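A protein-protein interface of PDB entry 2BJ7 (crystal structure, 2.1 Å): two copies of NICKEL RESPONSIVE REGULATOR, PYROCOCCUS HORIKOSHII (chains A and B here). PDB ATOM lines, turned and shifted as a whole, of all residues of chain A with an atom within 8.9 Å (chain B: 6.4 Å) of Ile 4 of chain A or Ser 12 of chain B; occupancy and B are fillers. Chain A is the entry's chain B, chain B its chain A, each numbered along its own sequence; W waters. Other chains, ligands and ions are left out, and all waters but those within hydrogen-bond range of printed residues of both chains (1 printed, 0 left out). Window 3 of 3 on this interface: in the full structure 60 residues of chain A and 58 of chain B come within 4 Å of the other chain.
The backbone NH (N) of Ile 8 of chain B lies within hydrogen-bond range of the backbone carbonyl oxygen (O) of Phe 6 of chain A. The side-chain hydroxyl (OG) of Ser 9 of chain B lies within hydrogen-bond range of the guanidinium group (NH1) of Arg 5 of chain A, 2.7 Å away. NH2 of Arg 35 of chain A is in hydrogen-bond range of O of Ser 9 of chain B (2.7 Å). The backbone NH (N) of Ile 4 of chain A sits at hydrogen-bond distance from the backbone carbonyl oxygen (O) of Ile 10 of chain B. The backbone carbonyl oxygen of Glu 2 of chain A is in hydrogen-bond range of the backbone NH of Ser 12 of chain B (2.8 Å).
Among the printed residues, pairs that only touch across the chains: Glu 2 of chain A with Pro 11 of chain B, Leu 3 of chain A with Ile 10 of chain B, Leu 3 of chain A with Pro 11 of chain B, Ile 4 of chain A with Ile 8 of chain B, Ile 4 of chain A with Ser 9 of chain B, Ile 4 of chain A with Ser 12 of chain B, Ile 4 of chain A with Leu 15 of chain B, Arg 5 of chain A with Ile 8 of chain B, Phe 6 of chain A with Ile 10 of chain B, Phe 6 of chain A with Leu 15 of chain B, Phe 6 of chain A with Arg 30 of chain B, Ile 42 of chain A with Leu 14 of chain B and Ile 42 of chain A with Lys 17 of chain B.
Of the printed residues of chain B, Ile 4 of chain A touches Ile 8 (3.7 Å), Ser 9 (3.5 Å), Ile 10 (2.9 Å), Ser 12 (3.6 Å) and Leu 15 (3.4 Å). Pro 11 of chain B touches two residues of chain A. Printed residues of chain B within 4 Å of Ile 42 of chain A: Leu 14 and Lys 17. Printed residues of chain A within 4 Å of Lys 17 of chain B: Ile 42 (3.4 Å). Printed residues of chain A within 4 Å of Ile 8 of chain B: Ile 4, Arg 5 and Phe 6. Of the printed residues of chain A, Leu 14 of chain B touches Ile 42 (3.5 Å). Of the printed residues of chain B, Glu 2 of chain A touches Pro 11 (3.5 Å) and Ser 12 (2.8 Å). The nearest printed residue of chain B that does not touch Ile 4 of chain A is Pro 11 of chain B (4.9 Å). The nearest printed residue of chain A that does not touch Leu 15 of chain B is Ile 42 of chain A (5.9 Å).
Of the 11 printed residues of chain B, 9 touch a printed residue of chain A. Printed residues of chain B that touch a printed residue of chain A: Ile 8, Ser 9, Ile 10, Pro 11, Ser 12, Leu 14, Leu 15, Lys 17 and Arg 30. Hydrophobic or aromatic side chains of chain B that line the printed part of chain A: Ile 8, Ile 10, Pro 11, Leu 14 and Leu 15. Of the 10 printed residues of chain A, 7 touch a printed residue of chain B. Printed residues of chain A that touch a printed residue of chain B: Glu 2, Leu 3, Ile 4, Arg 5, Phe 6, Arg 35 and Ile 42. Hydrophobic or aromatic side chains of chain A within 4 Å of the printed part of chain B: Leu 3, Ile 4, Phe 6 and Ile 42. Among the printed residues, 18 pairs touch across the chains.
No position is printed for both chains.
Water W1 lies within hydrogen-bond range of the side-chain hydroxyl (OG) of Ser 12 of chain B (2.6 Å) and the backbone NH (N) of Glu 2 of chain A (2.7 Å).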
ATOM      1  N   MET A   1     -10.322   3.520 -19.597  1.00  0.00           N
ATOM      2  CA  MET A   1      -9.907   3.702 -18.174  1.00  0.00           C
ATOM      3  C   MET A   1      -8.891   2.656 -17.737  1.00  0.00           C
ATOM      4  O   MET A   1      -9.021   1.469 -18.047  1.00  0.00           O
ATOM      5  CB  MET A   1     -11.127   3.631 -17.252  1.00  0.00           C
ATOM      6  CG  MET A   1     -10.780   3.492 -15.779  1.00  0.00           C
ATOM      7  SD  MET A   1      -9.817   4.876 -15.144  1.00  0.00           S
ATOM      8  CE  MET A   1     -11.136   5.960 -14.600  1.00  0.00           C
ATOM      9  N   GLU A   2      -7.873   3.106 -17.015  1.00  0.00           N
ATOM     10  CA  GLU A   2      -6.848   2.208 -16.520  1.00  0.00           C
ATOM     11  C   GLU A   2      -6.308   2.688 -15.182  1.00  0.00           C
ATOM     12  O   GLU A   2      -5.823   3.816 -15.056  1.00  0.00           O
ATOM     13  CB  GLU A   2      -5.696   2.095 -17.515  1.00  0.00           C
ATOM     14  CG  GLU A   2      -4.630   1.112 -17.067  1.00  0.00           C
ATOM     15  CD  GLU A   2      -3.441   1.065 -18.004  1.00  0.00           C
ATOM     16  OE1 GLU A   2      -2.763   2.102 -18.165  1.00  0.00           O
ATOM     17  OE2 GLU A   2      -3.184  -0.014 -18.581  1.00  0.00           O
ATOM     18  N   LEU A   3      -6.411   1.830 -14.176  1.00  0.00           N
ATOM     19  CA  LEU A   3      -5.899   2.164 -12.858  1.00  0.00           C
ATOM     20  C   LEU A   3      -4.535   1.519 -12.722  1.00  0.00           C
ATOM     21  O   LEU A   3      -4.357   0.352 -13.072  1.00  0.00           O
ATOM     22  CB  LEU A   3      -6.822   1.634 -11.766  1.00  0.00           C
ATOM     23  CG  LEU A   3      -8.151   2.355 -11.554  1.00  0.00           C
ATOM     24  CD1 LEU A   3      -8.882   1.713 -10.378  1.00  0.00           C
ATOM     25  CD2 LEU A   3      -7.895   3.834 -11.274  1.00  0.00           C
ATOM     26  N   ILE A   4      -3.565   2.287 -12.241  1.00  0.00           N
ATOM     27  CA  ILE A   4      -2.224   1.769 -12.040  1.00  0.00           C
ATOM     28  C   ILE A   4      -1.969   1.709 -10.542  1.00  0.00           C
ATOM     29  O   ILE A   4      -2.073   2.718  -9.842  1.00  0.00           O
ATOM     30  CB  ILE A   4      -1.175   2.659 -12.722  1.00  0.00           C
ATOM     31  CG1 ILE A   4      -1.310   2.520 -14.241  1.00  0.00           C
ATOM     32  CG2 ILE A   4       0.227   2.253 -12.274  1.00  0.00           C
ATOM     33  CD1 ILE A   4      -0.327   3.355 -15.031  1.00  0.00           C
ATOM     34  N   ARG A   5      -1.654   0.520 -10.044  1.00  0.00           N
ATOM     35  CA  ARG A   5      -1.414   0.360  -8.623  1.00  0.00           C
ATOM     36  C   ARG A   5       0.082   0.290  -8.362  1.00  0.00           C
ATOM     37  O   ARG A   5       0.798  -0.442  -9.036  1.00  0.00           O
ATOM     38  CB  ARG A   5      -2.124  -0.903  -8.125  1.00  0.00           C
ATOM     39  CG  ARG A   5      -2.211  -1.024  -6.617  1.00  0.00           C
ATOM     40  CD  ARG A   5      -3.223  -2.098  -6.204  1.00  0.00           C
ATOM     41  NE  ARG A   5      -3.347  -2.203  -4.751  1.00  0.00           N
ATOM     42  CZ  ARG A   5      -3.881  -1.270  -3.962  1.00  0.00           C
ATOM     43  NH1 ARG A   5      -4.363  -0.140  -4.470  1.00  0.00           N
ATOM     44  NH2 ARG A   5      -3.918  -1.464  -2.650  1.00  0.00           N
ATOM     45  N   PHE A   6       0.557   1.076  -7.401  1.00  0.00           N
ATOM     46  CA  PHE A   6       1.981   1.093  -7.069  1.00  0.00           C
ATOM     47  C   PHE A   6       2.169   1.325  -5.577  1.00  0.00           C
ATOM     48  O   PHE A   6       1.261   1.805  -4.896  1.00  0.00           O
ATOM     49  CB  PHE A   6       2.714   2.185  -7.862  1.00  0.00           C
ATOM     50  CG  PHE A   6       2.251   3.580  -7.553  1.00  0.00           C
ATOM     51  CD1 PHE A   6       1.080   4.080  -8.109  1.00  0.00           C
ATOM     52  CD2 PHE A   6       2.972   4.386  -6.673  1.00  0.00           C
ATOM     53  CE1 PHE A   6       0.629   5.365  -7.794  1.00  0.00           C
ATOM     54  CE2 PHE A   6       2.532   5.671  -6.348  1.00  0.00           C
ATOM     55  CZ  PHE A   6       1.357   6.161  -6.910  1.00  0.00           C
ATOM     56  N   SER A   7       3.349   0.978  -5.072  1.00  0.00           N
ATOM     57  CA  SER A   7       3.647   1.140  -3.655  1.00  0.00           C
ATOM     58  C   SER A   7       4.569   2.314  -3.390  1.00  0.00           C
ATOM     59  O   SER A   7       5.337   2.720  -4.259  1.00  0.00           O
ATOM     60  CB  SER A   7       4.301  -0.131  -3.098  1.00  0.00           C
ATOM     61  OG  SER A   7       3.387  -1.215  -3.095  1.00  0.00           O
ATOM     62  N   ARG A  35      -4.565  11.197  -3.676  1.00  0.00           N
ATOM     63  CA  ARG A  35      -4.878  11.522  -5.066  1.00  0.00           C
ATOM     64  C   ARG A  35      -5.180  13.020  -5.148  1.00  0.00           C
ATOM     65  O   ARG A  35      -4.843  13.673  -6.138  1.00  0.00           O
ATOM     66  CB  ARG A  35      -6.065  10.698  -5.585  1.00  0.00           C
ATOM     67  CG  ARG A  35      -5.685   9.266  -5.997  1.00  0.00           C
ATOM     68  CD  ARG A  35      -6.797   8.579  -6.809  1.00  0.00           C
ATOM     69  NE  ARG A  35      -7.941   8.229  -5.978  1.00  0.00           N
ATOM     70  CZ  ARG A  35      -7.978   7.180  -5.162  1.00  0.00           C
ATOM     71  NH1 ARG A  35      -9.059   6.949  -4.432  1.00  0.00           N
ATOM     72  NH2 ARG A  35      -6.943   6.351  -5.089  1.00  0.00           N
ATOM     73  N   ILE A  42      -0.273  18.874  -9.494  1.00  0.00           N
ATOM     74  CA  ILE A  42      -0.326  19.032 -10.945  1.00  0.00           C
ATOM     75  C   ILE A  42      -0.923  20.390 -11.339  1.00  0.00           C
ATOM     76  O   ILE A  42      -0.517  21.004 -12.330  1.00  0.00           O
ATOM     77  CB  ILE A  42      -1.170  17.904 -11.584  1.00  0.00           C
ATOM     78  CG1 ILE A  42      -0.456  16.560 -11.408  1.00  0.00           C
ATOM     79  CG2 ILE A  42      -1.422  18.196 -13.058  1.00  0.00           C
ATOM     80  CD1 ILE A  42      -1.241  15.395 -11.948  1.00  0.00           C
ATOM     81  N   VAL A 138      -8.595  14.248 -13.717  1.00  0.00           N
ATOM     82  CA  VAL A 138      -9.528  13.143 -13.550  1.00  0.00           C
ATOM     83  C   VAL A 138      -9.367  12.581 -12.138  1.00  0.00           C
ATOM     84  O   VAL A 138      -8.633  13.213 -11.339  1.00  0.00           O
ATOM     85  CB  VAL A 138      -9.279  12.010 -14.588  1.00  0.00           C
ATOM     86  CG1 VAL A 138      -9.506  12.535 -16.004  1.00  0.00           C
ATOM     87  CG2 VAL A 138      -7.867  11.461 -14.439  1.00  0.00           C
ATOM     88  OXT VAL A 138      -9.978  11.528 -11.846  1.00  0.00           O
ATOM     89  N   ILE B   8      -1.363   2.194  -3.484  1.00  0.00           N
ATOM     90  CA  ILE B   8      -2.406   3.128  -3.854  1.00  0.00           C
ATOM     91  C   ILE B   8      -2.702   2.918  -5.344  1.00  0.00           C
ATOM     92  O   ILE B   8      -1.806   2.562  -6.113  1.00  0.00           O
ATOM     93  CB  ILE B   8      -1.930   4.583  -3.603  1.00  0.00           C
ATOM     94  CG1 ILE B   8      -3.054   5.573  -3.879  1.00  0.00           C
ATOM     95  CG2 ILE B   8      -0.744   4.904  -4.500  1.00  0.00           C
ATOM     96  CD1 ILE B   8      -2.653   7.010  -3.605  1.00  0.00           C
ATOM     97  N   SER B   9      -3.956   3.113  -5.739  1.00  0.00           N
ATOM     98  CA  SER B   9      -4.357   2.972  -7.139  1.00  0.00           C
ATOM     99  C   SER B   9      -4.708   4.358  -7.652  1.00  0.00           C
ATOM    100  O   SER B   9      -5.382   5.123  -6.966  1.00  0.00           O
ATOM    101  CB  SER B   9      -5.572   2.048  -7.273  1.00  0.00           C
ATOM    102  OG  SER B   9      -5.228   0.719  -6.921  1.00  0.00           O
ATOM    103  N   ILE B  10      -4.249   4.673  -8.858  1.00  0.00           N
ATOM    104  CA  ILE B  10      -4.474   5.984  -9.454  1.00  0.00           C
ATOM    105  C   ILE B  10      -4.713   5.880 -10.957  1.00  0.00           C
ATOM    106  O   ILE B  10      -4.074   5.075 -11.635  1.00  0.00           O
ATOM    107  CB  ILE B  10      -3.258   6.902  -9.196  1.00  0.00           C
ATOM    108  CG1 ILE B  10      -3.422   8.229  -9.937  1.00  0.00           C
ATOM    109  CG2 ILE B  10      -1.993   6.204  -9.637  1.00  0.00           C
ATOM    110  CD1 ILE B  10      -2.278   9.191  -9.712  1.00  0.00           C
ATOM    111  N   PRO B  11      -5.648   6.679 -11.499  1.00  0.00           N
ATOM    112  CA  PRO B  11      -5.886   6.609 -12.944  1.00  0.00           C
ATOM    113  C   PRO B  11      -4.555   6.869 -13.641  1.00  0.00           C
ATOM    114  O   PRO B  11      -3.798   7.753 -13.234  1.00  0.00           O
ATOM    115  CB  PRO B  11      -6.895   7.726 -13.180  1.00  0.00           C
ATOM    116  CG  PRO B  11      -7.714   7.680 -11.926  1.00  0.00           C
ATOM    117  CD  PRO B  11      -6.655   7.532 -10.843  1.00  0.00           C
ATOM    118  N   SER B  12      -4.269   6.090 -14.678  1.00  0.00           N
ATOM    119  CA  SER B  12      -3.017   6.205 -15.416  1.00  0.00           C
ATOM    120  C   SER B  12      -2.698   7.606 -15.940  1.00  0.00           C
ATOM    121  O   SER B  12      -1.554   8.052 -15.851  1.00  0.00           O
ATOM    122  CB  SER B  12      -3.008   5.211 -16.583  1.00  0.00           C
ATOM    123  OG  SER B  12      -4.051   5.501 -17.495  1.00  0.00           O
ATOM    124  N   LYS B  13      -3.694   8.293 -16.494  1.00  0.00           N
ATOM    125  CA  LYS B  13      -3.468   9.638 -17.029  1.00  0.00           C
ATOM    126  C   LYS B  13      -2.886  10.548 -15.952  1.00  0.00           C
ATOM    127  O   LYS B  13      -1.919  11.271 -16.186  1.00  0.00           O
ATOM    128  CB  LYS B  13      -4.776  10.244 -17.542  1.00  0.00           C
ATOM    129  CG  LYS B  13      -5.473   9.430 -18.625  1.00  0.00           C
ATOM    130  CD  LYS B  13      -4.570   9.196 -19.826  1.00  0.00           C
ATOM    131  CE  LYS B  13      -5.292   8.383 -20.892  1.00  0.00           C
ATOM    132  NZ  LYS B  13      -4.415   8.106 -22.060  1.00  0.00           N
ATOM    133  N   LEU B  14      -3.479  10.491 -14.765  1.00  0.00           N
ATOM    134  CA  LEU B  14      -3.040  11.299 -13.640  1.00  0.00           C
ATOM    135  C   LEU B  14      -1.615  10.934 -13.211  1.00  0.00           C
ATOM    136  O   LEU B  14      -0.791  11.808 -12.940  1.00  0.00           O
ATOM    137  CB  LEU B  14      -4.003  11.102 -12.472  1.00  0.00           C
ATOM    138  CG  LEU B  14      -3.847  12.050 -11.292  1.00  0.00           C
ATOM    139  CD1 LEU B  14      -4.106  13.476 -11.763  1.00  0.00           C
ATOM    140  CD2 LEU B  14      -4.824  11.658 -10.187  1.00  0.00           C
ATOM    141  N   LEU B  15      -1.319   9.641 -13.158  1.00  0.00           N
ATOM    142  CA  LEU B  15       0.008   9.190 -12.755  1.00  0.00           C
ATOM    143  C   LEU B  15       1.079   9.564 -13.784  1.00  0.00           C
ATOM    144  O   LEU B  15       2.226   9.849 -13.423  1.00  0.00           O
ATOM    145  CB  LEU B  15      -0.001   7.675 -12.543  1.00  0.00           C
ATOM    146  CG  LEU B  15       1.291   7.061 -12.003  1.00  0.00           C
ATOM    147  CD1 LEU B  15       1.654   7.718 -10.673  1.00  0.00           C
ATOM    148  CD2 LEU B  15       1.104   5.553 -11.832  1.00  0.00           C
ATOM    149  N   GLU B  16       0.705   9.564 -15.060  1.00  0.00           N
ATOM    150  CA  GLU B  16       1.645   9.909 -16.127  1.00  0.00           C
ATOM    151  C   GLU B  16       2.155  11.327 -15.929  1.00  0.00           C
ATOM    152  O   GLU B  16       3.363  11.579 -15.927  1.00  0.00           O
ATOM    153  CB  GLU B  16       0.969   9.815 -17.495  1.00  0.00           C
ATOM    154  CG  GLU B  16       0.567   8.410 -17.911  1.00  0.00           C
ATOM    155  CD  GLU B  16      -0.134   8.379 -19.262  1.00  0.00           C
ATOM    156  OE1 GLU B  16      -0.509   7.274 -19.710  1.00  0.00           O
ATOM    157  OE2 GLU B  16      -0.311   9.457 -19.873  1.00  0.00           O
ATOM    158  N   LYS B  17       1.213  12.248 -15.760  1.00  0.00           N
ATOM    159  CA  LYS B  17       1.526  13.655 -15.562  1.00  0.00           C
ATOM    160  C   LYS B  17       2.372  13.850 -14.309  1.00  0.00           C
ATOM    161  O   LYS B  17       3.358  14.580 -14.329  1.00  0.00           O
ATOM    162  CB  LYS B  17       0.226  14.448 -15.446  1.00  0.00           C
ATOM    163  CG  LYS B  17       0.342  15.899 -15.841  1.00  0.00           C
ATOM    164  CD  LYS B  17      -1.042  16.529 -15.963  1.00  0.00           C
ATOM    165  CE  LYS B  17      -1.925  15.763 -16.948  1.00  0.00           C
ATOM    166  NZ  LYS B  17      -3.273  16.379 -17.102  1.00  0.00           N
ATOM    167  N   ARG B  30       8.803   8.318  -6.542  1.00  0.00           N
ATOM    168  CA  ARG B  30       7.484   8.811  -6.156  1.00  0.00           C
ATOM    169  C   ARG B  30       7.314   9.013  -4.658  1.00  0.00           C
ATOM    170  O   ARG B  30       6.612   9.926  -4.227  1.00  0.00           O
ATOM    171  CB  ARG B  30       6.406   7.851  -6.646  1.00  0.00           C
ATOM    172  CG  ARG B  30       6.340   7.707  -8.141  1.00  0.00           C
ATOM    173  CD  ARG B  30       5.362   6.622  -8.524  1.00  0.00           C
ATOM    174  NE  ARG B  30       5.210   6.502  -9.971  1.00  0.00           N
ATOM    175  CZ  ARG B  30       4.940   5.358 -10.592  1.00  0.00           C
ATOM    176  NH1 ARG B  30       4.801   4.242  -9.889  1.00  0.00           N
ATOM    177  NH2 ARG B  30       4.795   5.327 -11.910  1.00  0.00           N
HETATM  178  O   HOH W   1      -6.637   5.347 -17.991  1.00  0.00           O
